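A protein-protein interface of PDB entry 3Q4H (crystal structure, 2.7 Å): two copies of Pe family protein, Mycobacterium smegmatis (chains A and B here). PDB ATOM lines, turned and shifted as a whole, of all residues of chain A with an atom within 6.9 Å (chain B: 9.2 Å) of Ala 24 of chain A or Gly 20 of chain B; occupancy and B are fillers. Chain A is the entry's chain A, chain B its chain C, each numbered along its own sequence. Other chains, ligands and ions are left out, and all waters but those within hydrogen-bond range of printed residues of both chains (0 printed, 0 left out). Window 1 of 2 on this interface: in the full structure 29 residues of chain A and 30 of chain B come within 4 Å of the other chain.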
ATOM      1  N   PHE A  19     -26.723 -20.025 -14.765  1.00  0.00           N
ATOM      2  CA  PHE A  19     -27.431 -18.970 -15.495  1.00  0.00           C
ATOM      3  C   PHE A  19     -27.137 -17.601 -14.886  1.00  0.00           C
ATOM      4  O   PHE A  19     -26.941 -16.628 -15.612  1.00  0.00           O
ATOM      5  CB  PHE A  19     -28.951 -19.192 -15.524  1.00  0.00           C
ATOM      6  CG  PHE A  19     -29.689 -18.132 -16.305  1.00  0.00           C
ATOM      7  CD1 PHE A  19     -29.867 -18.255 -17.674  1.00  0.00           C
ATOM      8  CD2 PHE A  19     -30.167 -16.991 -15.676  1.00  0.00           C
ATOM      9  CE1 PHE A  19     -30.539 -17.266 -18.404  1.00  0.00           C
ATOM     10  CE2 PHE A  19     -30.837 -15.996 -16.404  1.00  0.00           C
ATOM     11  CZ  PHE A  19     -31.025 -16.141 -17.765  1.00  0.00           C
ATOM     12  N   GLY A  20     -27.122 -17.544 -13.554  1.00  0.00           N
ATOM     13  CA  GLY A  20     -26.852 -16.306 -12.838  1.00  0.00           C
ATOM     14  C   GLY A  20     -25.482 -15.746 -13.138  1.00  0.00           C
ATOM     15  O   GLY A  20     -25.313 -14.539 -13.230  1.00  0.00           O
ATOM     16  N   ALA A  21     -24.506 -16.635 -13.288  1.00  0.00           N
ATOM     17  CA  ALA A  21     -23.160 -16.240 -13.646  1.00  0.00           C
ATOM     18  C   ALA A  21     -23.141 -15.596 -15.027  1.00  0.00           C
ATOM     19  O   ALA A  21     -22.585 -14.512 -15.194  1.00  0.00           O
ATOM     20  CB  ALA A  21     -22.235 -17.432 -13.608  1.00  0.00           C
ATOM     21  N   LYS A  22     -23.758 -16.250 -16.011  1.00  0.00           N
ATOM     22  CA  LYS A  22     -23.774 -15.721 -17.382  1.00  0.00           C
ATOM     23  C   LYS A  22     -24.512 -14.393 -17.458  1.00  0.00           C
ATOM     24  O   LYS A  22     -24.153 -13.529 -18.245  1.00  0.00           O
ATOM     25  CB  LYS A  22     -24.416 -16.706 -18.358  1.00  0.00           C
ATOM     26  CG  LYS A  22     -23.655 -18.009 -18.536  1.00  0.00           C
ATOM     27  CD  LYS A  22     -24.364 -18.920 -19.523  1.00  0.00           C
ATOM     28  CE  LYS A  22     -23.580 -20.187 -19.806  1.00  0.00           C
ATOM     29  NZ  LYS A  22     -24.217 -20.925 -20.923  1.00  0.00           N
ATOM     30  N   ALA A  23     -25.546 -14.230 -16.644  1.00  0.00           N
ATOM     31  CA  ALA A  23     -26.228 -12.955 -16.568  1.00  0.00           C
ATOM     32  C   ALA A  23     -25.215 -11.901 -16.136  1.00  0.00           C
ATOM     33  O   ALA A  23     -25.071 -10.861 -16.784  1.00  0.00           O
ATOM     34  CB  ALA A  23     -27.399 -13.020 -15.608  1.00  0.00           C
ATOM     35  N   ALA A  24     -24.475 -12.181 -15.068  1.00  0.00           N
ATOM     36  CA  ALA A  24     -23.484 -11.221 -14.586  1.00  0.00           C
ATOM     37  C   ALA A  24     -22.420 -10.978 -15.648  1.00  0.00           C
ATOM     38  O   ALA A  24     -21.961  -9.861 -15.813  1.00  0.00           O
ATOM     39  CB  ALA A  24     -22.857 -11.694 -13.312  1.00  0.00           C
ATOM     40  N   LEU A  25     -22.059 -12.015 -16.394  1.00  0.00           N
ATOM     41  CA  LEU A  25     -21.016 -11.890 -17.407  1.00  0.00           C
ATOM     42  C   LEU A  25     -21.461 -11.062 -18.617  1.00  0.00           C
ATOM     43  O   LEU A  25     -20.639 -10.372 -19.235  1.00  0.00           O
ATOM     44  CB  LEU A  25     -20.500 -13.272 -17.826  1.00  0.00           C
ATOM     45  CG  LEU A  25     -19.624 -13.969 -16.767  1.00  0.00           C
ATOM     46  CD1 LEU A  25     -19.113 -15.316 -17.259  1.00  0.00           C
ATOM     47  CD2 LEU A  25     -18.459 -13.082 -16.355  1.00  0.00           C
ATOM     48  N   MET A  26     -22.752 -11.106 -18.940  1.00  0.00           N
ATOM     49  CA  MET A  26     -23.318 -10.180 -19.918  1.00  0.00           C
ATOM     50  C   MET A  26     -23.163  -8.724 -19.441  1.00  0.00           C
ATOM     51  O   MET A  26     -22.596  -7.901 -20.150  1.00  0.00           O
ATOM     52  CB  MET A  26     -24.788 -10.498 -20.179  1.00  0.00           C
ATOM     53  CG  MET A  26     -25.496  -9.529 -21.132  1.00  0.00           C
ATOM     54  SD  MET A  26     -24.789  -9.477 -22.974  1.00  0.00           S
ATOM     55  CE  MET A  26     -25.328 -11.240 -23.554  1.00  0.00           C
ATOM     56  N   ARG A  27     -23.645  -8.416 -18.236  1.00  0.00           N
ATOM     57  CA  ARG A  27     -23.486  -7.081 -17.666  1.00  0.00           C
ATOM     58  C   ARG A  27     -22.029  -6.616 -17.746  1.00  0.00           C
ATOM     59  O   ARG A  27     -21.755  -5.435 -17.958  1.00  0.00           O
ATOM     60  CB  ARG A  27     -23.908  -7.049 -16.196  1.00  0.00           C
ATOM     61  CG  ARG A  27     -25.351  -7.434 -15.890  1.00  0.00           C
ATOM     62  CD  ARG A  27     -25.669  -7.146 -14.430  1.00  0.00           C
ATOM     63  NE  ARG A  27     -26.696  -8.034 -13.883  1.00  0.00           N
ATOM     64  CZ  ARG A  27     -28.004  -7.784 -13.882  1.00  0.00           C
ATOM     65  NH1 ARG A  27     -28.494  -6.676 -14.435  1.00  0.00           N
ATOM     66  NH2 ARG A  27     -28.839  -8.658 -13.339  1.00  0.00           N
ATOM     67  N   SER A  28     -21.107  -7.556 -17.545  1.00  0.00           N
ATOM     68  CA  SER A  28     -19.670  -7.289 -17.613  1.00  0.00           C
ATOM     69  C   SER A  28     -19.209  -6.994 -19.044  1.00  0.00           C
ATOM     70  O   SER A  28     -18.435  -6.072 -19.276  1.00  0.00           O
ATOM     71  CB  SER A  28     -18.894  -8.485 -17.052  1.00  0.00           C
ATOM     72  OG  SER A  28     -17.511  -8.190 -16.946  1.00  0.00           O
ATOM     73  N   THR A  29     -19.688  -7.795 -19.992  1.00  0.00           N
ATOM     74  CA  THR A  29     -19.400  -7.594 -21.406  1.00  0.00           C
ATOM     75  C   THR A  29     -19.929  -6.268 -21.922  1.00  0.00           C
ATOM     76  O   THR A  29     -19.228  -5.582 -22.659  1.00  0.00           O
ATOM     77  CB  THR A  29     -20.019  -8.703 -22.228  1.00  0.00           C
ATOM     78  OG1 THR A  29     -19.476  -9.952 -21.786  1.00  0.00           O
ATOM     79  CG2 THR A  29     -19.736  -8.508 -23.720  1.00  0.00           C
ATOM     80  N   LEU A  70     -32.366  -8.732 -17.285  1.00  0.00           N
ATOM     81  CA  LEU A  70     -31.566  -9.701 -16.546  1.00  0.00           C
ATOM     82  C   LEU A  70     -32.005  -9.735 -15.080  1.00  0.00           C
ATOM     83  O   LEU A  70     -32.069 -10.805 -14.471  1.00  0.00           O
ATOM     84  CB  LEU A  70     -30.077  -9.376 -16.644  1.00  0.00           C
ATOM     85  CG  LEU A  70     -29.410  -9.549 -18.015  1.00  0.00           C
ATOM     86  CD1 LEU A  70     -27.968  -8.985 -18.019  1.00  0.00           C
ATOM     87  CD2 LEU A  70     -29.415 -11.016 -18.437  1.00  0.00           C
ATOM     88  N   GLN A  74     -32.902 -13.178 -13.157  1.00  0.00           N
ATOM     89  CA  GLN A  74     -32.216 -13.565 -11.931  1.00  0.00           C
ATOM     90  C   GLN A  74     -33.182 -14.030 -10.852  1.00  0.00           C
ATOM     91  O   GLN A  74     -32.957 -15.063 -10.211  1.00  0.00           O
ATOM     92  CB  GLN A  74     -31.358 -12.415 -11.393  1.00  0.00           C
ATOM     93  CG  GLN A  74     -30.124 -12.057 -12.247  1.00  0.00           C
ATOM     94  CD  GLN A  74     -29.008 -13.096 -12.181  1.00  0.00           C
ATOM     95  OE1 GLN A  74     -29.264 -14.286 -12.107  1.00  0.00           O
ATOM     96  NE2 GLN A  74     -27.765 -12.638 -12.221  1.00  0.00           N
ATOM     97  N   ASP A  79     -29.380 -16.182 -10.189  1.00  0.00           N
ATOM     98  CA  ASP A  79     -28.653 -16.082  -8.925  1.00  0.00           C
ATOM     99  C   ASP A  79     -29.563 -16.104  -7.703  1.00  0.00           C
ATOM    100  O   ASP A  79     -29.290 -16.831  -6.748  1.00  0.00           O
ATOM    101  CB  ASP A  79     -27.797 -14.823  -8.876  1.00  0.00           C
ATOM    102  CG  ASP A  79     -26.817 -14.853  -7.734  1.00  0.00           C
ATOM    103  OD1 ASP A  79     -25.901 -15.694  -7.791  1.00  0.00           O
ATOM    104  OD2 ASP A  79     -26.956 -14.063  -6.769  1.00  0.00           O
ATOM    105  N   LEU B  12     -16.500   0.572 -12.793  1.00  0.00           N
ATOM    106  CA  LEU B  12     -17.229   0.126 -11.599  1.00  0.00           C
ATOM    107  C   LEU B  12     -18.263  -0.949 -11.929  1.00  0.00           C
ATOM    108  O   LEU B  12     -18.316  -1.991 -11.280  1.00  0.00           O
ATOM    109  CB  LEU B  12     -17.912   1.312 -10.900  1.00  0.00           C
ATOM    110  CG  LEU B  12     -18.635   1.062  -9.557  1.00  0.00           C
ATOM    111  CD1 LEU B  12     -17.801   0.231  -8.579  1.00  0.00           C
ATOM    112  CD2 LEU B  12     -19.038   2.394  -8.913  1.00  0.00           C
ATOM    113  N   ILE B  13     -19.082  -0.679 -12.940  1.00  0.00           N
ATOM    114  CA  ILE B  13     -20.062  -1.649 -13.434  1.00  0.00           C
ATOM    115  C   ILE B  13     -19.392  -2.986 -13.792  1.00  0.00           C
ATOM    116  O   ILE B  13     -19.838  -4.044 -13.360  1.00  0.00           O
ATOM    117  CB  ILE B  13     -20.805  -1.114 -14.676  1.00  0.00           C
ATOM    118  CG1 ILE B  13     -21.727   0.052 -14.301  1.00  0.00           C
ATOM    119  CG2 ILE B  13     -21.600  -2.226 -15.326  1.00  0.00           C
ATOM    120  CD1 ILE B  13     -22.205   0.894 -15.499  1.00  0.00           C
ATOM    121  N   ALA B  14     -18.315  -2.933 -14.568  1.00  0.00           N
ATOM    122  CA  ALA B  14     -17.589  -4.141 -14.941  1.00  0.00           C
ATOM    123  C   ALA B  14     -17.149  -4.929 -13.690  1.00  0.00           C
ATOM    124  O   ALA B  14     -17.469  -6.109 -13.553  1.00  0.00           O
ATOM    125  CB  ALA B  14     -16.382  -3.786 -15.828  1.00  0.00           C
ATOM    126  N   SER B  15     -16.443  -4.268 -12.775  1.00  0.00           N
ATOM    127  CA  SER B  15     -15.942  -4.929 -11.568  1.00  0.00           C
ATOM    128  C   SER B  15     -17.050  -5.505 -10.690  1.00  0.00           C
ATOM    129  O   SER B  15     -16.900  -6.590 -10.120  1.00  0.00           O
ATOM    130  CB  SER B  15     -15.108  -3.961 -10.739  1.00  0.00           C
ATOM    131  OG  SER B  15     -14.023  -3.466 -11.499  1.00  0.00           O
ATOM    132  N   GLU B  16     -18.158  -4.787 -10.575  1.00  0.00           N
ATOM    133  CA  GLU B  16     -19.279  -5.277  -9.783  1.00  0.00           C
ATOM    134  C   GLU B  16     -19.935  -6.479 -10.471  1.00  0.00           C
ATOM    135  O   GLU B  16     -20.410  -7.405  -9.805  1.00  0.00           O
ATOM    136  CB  GLU B  16     -20.279  -4.150  -9.479  1.00  0.00           C
ATOM    137  CG  GLU B  16     -19.741  -3.128  -8.455  1.00  0.00           C
ATOM    138  CD  GLU B  16     -20.790  -2.116  -7.982  1.00  0.00           C
ATOM    139  OE1 GLU B  16     -21.715  -1.780  -8.750  1.00  0.00           O
ATOM    140  OE2 GLU B  16     -20.687  -1.643  -6.830  1.00  0.00           O
ATOM    141  N   ALA B  17     -19.919  -6.487 -11.801  1.00  0.00           N
ATOM    142  CA  ALA B  17     -20.423  -7.633 -12.553  1.00  0.00           C
ATOM    143  C   ALA B  17     -19.531  -8.864 -12.336  1.00  0.00           C
ATOM    144  O   ALA B  17     -20.031  -9.970 -12.081  1.00  0.00           O
ATOM    145  CB  ALA B  17     -20.526  -7.296 -14.039  1.00  0.00           C
ATOM    146  N   ASN B  18     -18.216  -8.659 -12.422  1.00  0.00           N
ATOM    147  CA  ASN B  18     -17.250  -9.748 -12.255  1.00  0.00           C
ATOM    148  C   ASN B  18     -17.350 -10.410 -10.885  1.00  0.00           C
ATOM    149  O   ASN B  18     -17.365 -11.635 -10.793  1.00  0.00           O
ATOM    150  CB  ASN B  18     -15.824  -9.262 -12.507  1.00  0.00           C
ATOM    151  CG  ASN B  18     -15.637  -8.695 -13.906  1.00  0.00           C
ATOM    152  OD1 ASN B  18     -16.490  -8.876 -14.773  1.00  0.00           O
ATOM    153  ND2 ASN B  18     -14.526  -7.995 -14.124  1.00  0.00           N
ATOM    154  N   PHE B  19     -17.433  -9.607  -9.826  1.00  0.00           N
ATOM    155  CA  PHE B  19     -17.689 -10.146  -8.491  1.00  0.00           C
ATOM    156  C   PHE B  19     -19.001 -10.908  -8.478  1.00  0.00           C
ATOM    157  O   PHE B  19     -19.104 -11.949  -7.841  1.00  0.00           O
ATOM    158  CB  PHE B  19     -17.744  -9.037  -7.424  1.00  0.00           C
ATOM    159  CG  PHE B  19     -18.129  -9.536  -6.044  1.00  0.00           C
ATOM    160  CD1 PHE B  19     -19.461  -9.791  -5.719  1.00  0.00           C
ATOM    161  CD2 PHE B  19     -17.163  -9.765  -5.082  1.00  0.00           C
ATOM    162  CE1 PHE B  19     -19.815 -10.257  -4.459  1.00  0.00           C
ATOM    163  CE2 PHE B  19     -17.513 -10.232  -3.810  1.00  0.00           C
ATOM    164  CZ  PHE B  19     -18.839 -10.478  -3.503  1.00  0.00           C
ATOM    165  N   GLY B  20     -20.007 -10.374  -9.161  1.00  0.00           N
ATOM    166  CA  GLY B  20     -21.321 -11.014  -9.224  1.00  0.00           C
ATOM    167  C   GLY B  20     -21.320 -12.368  -9.906  1.00  0.00           C
ATOM    168  O   GLY B  20     -22.088 -13.256  -9.539  1.00  0.00           O
ATOM    169  N   ALA B  21     -20.457 -12.516 -10.909  1.00  0.00           N
ATOM    170  CA  ALA B  21     -20.283 -13.789 -11.614  1.00  0.00           C
ATOM    171  C   ALA B  21     -19.649 -14.811 -10.680  1.00  0.00           C
ATOM    172  O   ALA B  21     -20.069 -15.970 -10.650  1.00  0.00           O
ATOM    173  CB  ALA B  21     -19.421 -13.603 -12.849  1.00  0.00           C
ATOM    174  N   LYS B  22     -18.645 -14.363  -9.920  1.00  0.00           N
ATOM    175  CA  LYS B  22     -17.934 -15.224  -8.981  1.00  0.00           C
ATOM    176  C   LYS B  22     -18.833 -15.721  -7.855  1.00  0.00           C
ATOM    177  O   LYS B  22     -18.801 -16.906  -7.531  1.00  0.00           O
ATOM    178  CB  LYS B  22     -16.707 -14.518  -8.402  1.00  0.00           C
ATOM    179  CG  LYS B  22     -15.501 -14.643  -9.288  1.00  0.00           C
ATOM    180  CD  LYS B  22     -14.321 -13.873  -8.751  1.00  0.00           C
ATOM    181  CE  LYS B  22     -13.132 -14.013  -9.679  1.00  0.00           C
ATOM    182  NZ  LYS B  22     -11.847 -13.644  -8.989  1.00  0.00           N
ATOM    183  N   ALA B  23     -19.610 -14.816  -7.259  1.00  0.00           N
ATOM    184  CA  ALA B  23     -20.624 -15.191  -6.267  1.00  0.00           C
ATOM    185  C   ALA B  23     -21.546 -16.290  -6.811  1.00  0.00           C
ATOM    186  O   ALA B  23     -21.871 -17.240  -6.105  1.00  0.00           O
ATOM    187  CB  ALA B  23     -21.443 -13.979  -5.860  1.00  0.00           C
ATOM    188  N   ALA B  24     -21.957 -16.169  -8.068  1.00  0.00           N
ATOM    189  CA  ALA B  24     -22.835 -17.150  -8.671  1.00  0.00           C
ATOM    190  C   ALA B  24     -22.099 -18.482  -8.936  1.00  0.00           C
ATOM    191  O   ALA B  24     -22.668 -19.564  -8.760  1.00  0.00           O
ATOM    192  CB  ALA B  24     -23.456 -16.586  -9.947  1.00  0.00           C
ATOM    193  N   LEU B  25     -20.834 -18.415  -9.341  1.00  0.00           N
ATOM    194  CA  LEU B  25     -20.055 -19.636  -9.559  1.00  0.00           C
ATOM    195  C   LEU B  25     -19.798 -20.356  -8.246  1.00  0.00           C
ATOM    196  O   LEU B  25     -19.828 -21.590  -8.199  1.00  0.00           O
ATOM    197  CB  LEU B  25     -18.739 -19.337 -10.261  1.00  0.00           C
ATOM    198  CG  LEU B  25     -18.887 -18.921 -11.723  1.00  0.00           C
ATOM    199  CD1 LEU B  25     -17.553 -18.437 -12.270  1.00  0.00           C
ATOM    200  CD2 LEU B  25     -19.449 -20.051 -12.566  1.00  0.00           C
ATOM    201  N   MET B  26     -19.559 -19.593  -7.183  1.00  0.00           N
ATOM    202  CA  MET B  26     -19.453 -20.171  -5.851  1.00  0.00           C
ATOM    203  C   MET B  26     -20.711 -20.980  -5.538  1.00  0.00           C
ATOM    204  O   MET B  26     -20.619 -22.148  -5.185  1.00  0.00           O
ATOM    205  CB  MET B  26     -19.244 -19.080  -4.797  1.00  0.00           C
ATOM    206  CG  MET B  26     -19.285 -19.574  -3.338  1.00  0.00           C
ATOM    207  SD  MET B  26     -18.018 -21.021  -2.855  1.00  0.00           S
ATOM    208  CE  MET B  26     -16.450 -19.961  -2.362  1.00  0.00           C
ATOM    209  N   ARG B  27     -21.880 -20.352  -5.684  1.00  0.00           N
ATOM    210  CA  ARG B  27     -23.151 -21.028  -5.449  1.00  0.00           C
ATOM    211  C   ARG B  27     -23.236 -22.322  -6.235  1.00  0.00           C
ATOM    212  O   ARG B  27     -23.617 -23.369  -5.704  1.00  0.00           O
ATOM    213  CB  ARG B  27     -24.322 -20.155  -5.865  1.00  0.00           C
ATOM    214  CG  ARG B  27     -24.520 -18.875  -5.074  1.00  0.00           C
ATOM    215  CD  ARG B  27     -25.887 -18.263  -5.424  1.00  0.00           C
ATOM    216  NE  ARG B  27     -25.955 -16.815  -5.228  1.00  0.00           N
ATOM    217  CZ  ARG B  27     -26.284 -16.206  -4.089  1.00  0.00           C
ATOM    218  NH1 ARG B  27     -26.545 -16.898  -2.980  1.00  0.00           N
ATOM    219  NH2 ARG B  27     -26.328 -14.875  -4.056  1.00  0.00           N
ATOM    220  N   LEU B  70     -23.747 -14.070   0.371  1.00  0.00           N
ATOM    221  CA  LEU B  70     -23.598 -13.629  -1.022  1.00  0.00           C
ATOM    222  C   LEU B  70     -24.786 -12.737  -1.473  1.00  0.00           C
ATOM    223  O   LEU B  70     -24.593 -11.754  -2.204  1.00  0.00           O
ATOM    224  CB  LEU B  70     -23.405 -14.827  -1.960  1.00  0.00           C
ATOM    225  CG  LEU B  70     -22.097 -15.634  -1.810  1.00  0.00           C
ATOM    226  CD1 LEU B  70     -22.150 -16.918  -2.639  1.00  0.00           C
ATOM    227  CD2 LEU B  70     -20.844 -14.820  -2.168  1.00  0.00           C
ATOM    228  N   ALA B  73     -23.717  -9.384  -0.407  1.00  0.00           N
ATOM    229  CA  ALA B  73     -22.676  -8.829  -1.269  1.00  0.00           C
ATOM    230  C   ALA B  73     -23.215  -8.449  -2.662  1.00  0.00           C
ATOM    231  O   ALA B  73     -22.847  -7.394  -3.197  1.00  0.00           O
ATOM    232  CB  ALA B  73     -21.502  -9.781  -1.380  1.00  0.00           C
ATOM    233  N   GLN B  74     -24.090  -9.281  -3.237  1.00  0.00           N
ATOM    234  CA  GLN B  74     -24.696  -8.975  -4.551  1.00  0.00           C
ATOM    235  C   GLN B  74     -25.437  -7.631  -4.536  1.00  0.00           C
ATOM    236  O   GLN B  74     -25.356  -6.854  -5.494  1.00  0.00           O
ATOM    237  CB  GLN B  74     -25.660 -10.080  -5.009  1.00  0.00           C
ATOM    238  CG  GLN B  74     -25.028 -11.458  -5.266  1.00  0.00           C
ATOM    239  CD  GLN B  74     -24.376 -11.590  -6.622  1.00  0.00           C
ATOM    240  OE1 GLN B  74     -23.545 -10.772  -7.000  1.00  0.00           O
ATOM    241  NE2 GLN B  74     -24.733 -12.634  -7.356  1.00  0.00           N
ATOM    242  N   LEU B  75     -26.163  -7.371  -3.452  1.00  0.00           N
ATOM    243  CA  LEU B  75     -26.838  -6.085  -3.264  1.00  0.00           C
ATOM    244  C   LEU B  75     -25.854  -4.907  -3.118  1.00  0.00           C
ATOM    245  O   LEU B  75     -26.112  -3.814  -3.621  1.00  0.00           O
ATOM    246  CB  LEU B  75     -27.761  -6.139  -2.040  1.00  0.00           C
ATOM    247  CG  LEU B  75     -29.058  -6.958  -2.185  1.00  0.00           C
ATOM    248  CD1 LEU B  75     -29.691  -7.201  -0.826  1.00  0.00           C
ATOM    249  CD2 LEU B  75     -30.069  -6.276  -3.128  1.00  0.00           C
ATOM    250  N   ILE B  77     -22.089  -4.861  -3.787  1.00  0.00           N
ATOM    251  CA  ILE B  77     -21.036  -4.717  -4.812  1.00  0.00           C
ATOM    252  C   ILE B  77     -21.067  -5.765  -5.946  1.00  0.00           C
ATOM    253  O   ILE B  77     -20.108  -5.895  -6.691  1.00  0.00           O
ATOM    254  CB  ILE B  77     -19.613  -4.711  -4.174  1.00  0.00           C
ATOM    255  CG1 ILE B  77     -19.418  -5.915  -3.252  1.00  0.00           C
ATOM    256  CG2 ILE B  77     -19.375  -3.444  -3.394  1.00  0.00           C
ATOM    257  CD1 ILE B  77     -17.980  -6.093  -2.816  1.00  0.00           C
ATOM    258  N   GLY B  78     -22.175  -6.474  -6.107  1.00  0.00           N
ATOM    259  CA  GLY B  78     -22.251  -7.551  -7.086  1.00  0.00           C
ATOM    260  C   GLY B  78     -23.218  -7.282  -8.217  1.00  0.00           C
ATOM    261  O   GLY B  78     -23.200  -6.214  -8.818  1.00  0.00           O
ATOM    262  N   ASP B  79     -24.072  -8.260  -8.495  1.00  0.00           N
ATOM    263  CA  ASP B  79     -24.928  -8.259  -9.676  1.00  0.00           C
ATOM    264  C   ASP B  79     -26.041  -7.223  -9.604  1.00  0.00           C
ATOM    265  O   ASP B  79     -26.356  -6.574 -10.607  1.00  0.00           O
ATOM    266  CB  ASP B  79     -25.539  -9.643  -9.856  1.00  0.00           C
ATOM    267  CG  ASP B  79     -26.227  -9.808 -11.187  1.00  0.00           C
ATOM    268  OD1 ASP B  79     -25.532  -9.825 -12.224  1.00  0.00           O
ATOM    269  OD2 ASP B  79     -27.467  -9.948 -11.196  1.00  0.00           O
ATOM    270  N   ALA B  80     -26.653  -7.078  -8.431  1.00  0.00           N
ATOM    271  CA  ALA B  80     -27.696  -6.074  -8.238  1.00  0.00           C
ATOM    272  C   ALA B  80     -27.065  -4.688  -8.237  1.00  0.00           C
ATOM    273  O   ALA B  80     -27.536  -3.791  -8.931  1.00  0.00           O
ATOM    274  CB  ALA B  80     -28.437  -6.326  -6.954  1.00  0.00           C
ATOM    275  N   ALA B  81     -25.982  -4.535  -7.475  1.00  0.00           N
ATOM    276  CA  ALA B  81     -25.244  -3.272  -7.389  1.00  0.00           C
ATOM    277  C   ALA B  81     -24.896  -2.724  -8.772  1.00  0.00           C
ATOM    278  O   ALA B  81     -25.217  -1.576  -9.089  1.00  0.00           O
ATOM    279  CB  ALA B  81     -23.974  -3.458  -6.571  1.00  0.00           C
ATOM    280  N   SER B  82     -24.260  -3.554  -9.596  1.00  0.00           N
ATOM    281  CA  SER B  82     -23.860  -3.137 -10.935  1.00  0.00           C
ATOM    282  C   SER B  82     -25.063  -2.873 -11.835  1.00  0.00           C
ATOM    283  O   SER B  82     -25.028  -1.965 -12.658  1.00  0.00           O
ATOM    284  CB  SER B  82     -22.939  -4.168 -11.588  1.00  0.00           C
ATOM    285  OG  SER B  82     -23.653  -5.038 -12.437  1.00  0.00           O
ATOM    286  N   SER B  83     -26.125  -3.657 -11.685  1.00  0.00           N
ATOM    287  CA  SER B  83     -27.354  -3.392 -12.426  1.00  0.00           C
ATOM    288  C   SER B  83     -27.910  -2.019 -12.072  1.00  0.00           C
ATOM    289  O   SER B  83     -28.266  -1.242 -12.959  1.00  0.00           O
ATOM    290  CB  SER B  83     -28.412  -4.452 -12.147  1.00  0.00           C
ATOM    291  OG  SER B  83     -29.535  -4.265 -12.998  1.00  0.00           O
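The guanidinium group of Arg 27 of chain A is in salt-bridge range of the side-chain carboxylate of Asp 79 of chain B.
The guanidinium group of Arg 27 of chain A is in hydrogen-bond range of the side-chain hydroxyl of Ser 83 of chain B (3.0 Å).
The side-chain amide oxygen (OD1) of Asn 18 of chain B sits at hydrogen-bond distance from the side-chain hydroxyl (OG) of Ser 28 of chain A, at 2.5 Å.
The side-chain amide nitrogen (NE2) of Gln 74 of chain A lies within hydrogen-bond range of the side-chain carboxylate (OD2) of Asp 79 of chain B.
The side-chain carboxylate (OD1) of Asp 79 of chain A is in salt-bridge range of the guanidinium group (NE) of Arg 27 of chain B (2.8 Å).
OD2 of Asp 79 of chain A lies within hydrogen-bond range of NE2 of Gln 74 of chain B, 2.7 Å away.
No residue of chain B comes within 4 Å of Ala 23 of chain A.
Of the printed residues of chain B, Gln 74 of chain A touches Asp 79 (2.9 Å).
Printed residues of chain B within 4 Å of Asp 79 of chain A: Ala 24, Arg 27 and Gln 74.
Of the printed residues of chain A, Ala 14 of chain B touches Ser 28 (3.98 Å).
Printed residues of chain A within 4 Å of Gly 20 of chain B: Ala 24.
Met 26 of chain B touches none of the printed residues of chain A.
Of the printed residues of chain A, Ser 82 of chain B touches Arg 27 (3.5 Å).
The nearest printed residue of chain B that does not touch Gln 74 of chain A is Gln 74 of chain B (5.7 Å).
O of Gly 20 of chain A is in hydrogen-bond range of NE2 of Gln 74 of chain A.
The backbone carbonyl oxygen (O) of Leu 25 of chain A is in hydrogen-bond range of the side-chain hydroxyl (OG1) of Thr 29 of chain A, 2.8 Å away.
The side-chain amide oxygen (OE1) of Gln 74 of chain A lies within hydrogen-bond range of the backbone NH (N) of Asp 79 of chain A, at 2.7 Å.
O of Ala 14 of chain B sits close to OD1 of Asn 18 of chain B.
The side-chain carboxylate (OE1) of Glu 16 of chain B is in hydrogen-bond range of the backbone NH (N) of Ser 82 of chain B (3.2 Å).
O of Gln 74 of chain B is in hydrogen-bond range of N of Ala 81 of chain B (3.1 Å).
Ala 21 of chain B touches its own counterpart, Ala 21 of chain A.
Ala 21 of chain A touches Ala 24 of chain B, and with the chains exchanged Ala 24 of chain A touches Ala 21 of chain B.
Ala 24 of chain A touches Asp 79 of chain B, and with the chains exchanged Asp 79 of chain A touches Ala 24 of chain B.
Arg 27 of chain A touches Asp 79 of chain B, and with the chains exchanged Asp 79 of chain A touches Arg 27 of chain B.
Positions printed for both chains: 19, 20, 21, 22, 23, 24, 25, 26, 27, 70, 74 and 79.
Of the 19 pairs that touch across the chains among the printed residues, 13 have their exchanged pair printed and touching as well.
Of the 14 printed residues of chain A, 8 touch a printed residue of chain B.
Hydrophobic or aromatic side chains of chain A within 4 Å of the printed part of chain B: Ala 21, Ala 24 and Leu 25.
Of the 27 printed residues of chain B, 12 touch a printed residue of chain A.
Among the printed residues, 19 pairs touch across the chains.
Among the printed residues, Asp or Glu carboxylates within 4 Å of a Lys or Arg side-chain nitrogen of the other chain: Arg 27 of chain A with Asp 79 of chain B (2.7 Å) and Asp 79 of chain A with Arg 27 of chain B (2.8 Å).
Among the printed residues, pairs that only touch across the chains: Asp 79 of chain A with Ala 24 of chain B (3.4 Å), Ala 24 of chain A with Asp 79 of chain B (3.4 Å), Ala 24 of chain A with Ala 17 of chain B (3.4 Å), Ala 24 of chain A with Ala 21 of chain B (3.5 Å), Ala 21 of chain A with Ala 24 of chain B (3.5 Å), Arg 27 of chain A with Ser 82 of chain B (3.5 Å), Ser 28 of chain A with Ala 17 of chain B (3.6 Å), Leu 25 of chain A with Ala 21 of chain B (3.7 Å), Ala 24 of chain A with Gly 20 of chain B (3.8 Å), Gly 20 of chain A with Ala 24 of chain B (3.9 Å), Ala 21 of chain A with Ala 21 of chain B (3.9 Å), Ala 21 of chain A with Leu 25 of chain B (3.96 Å) and Ser 28 of chain A with Ala 14 of chain B (3.98 Å).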
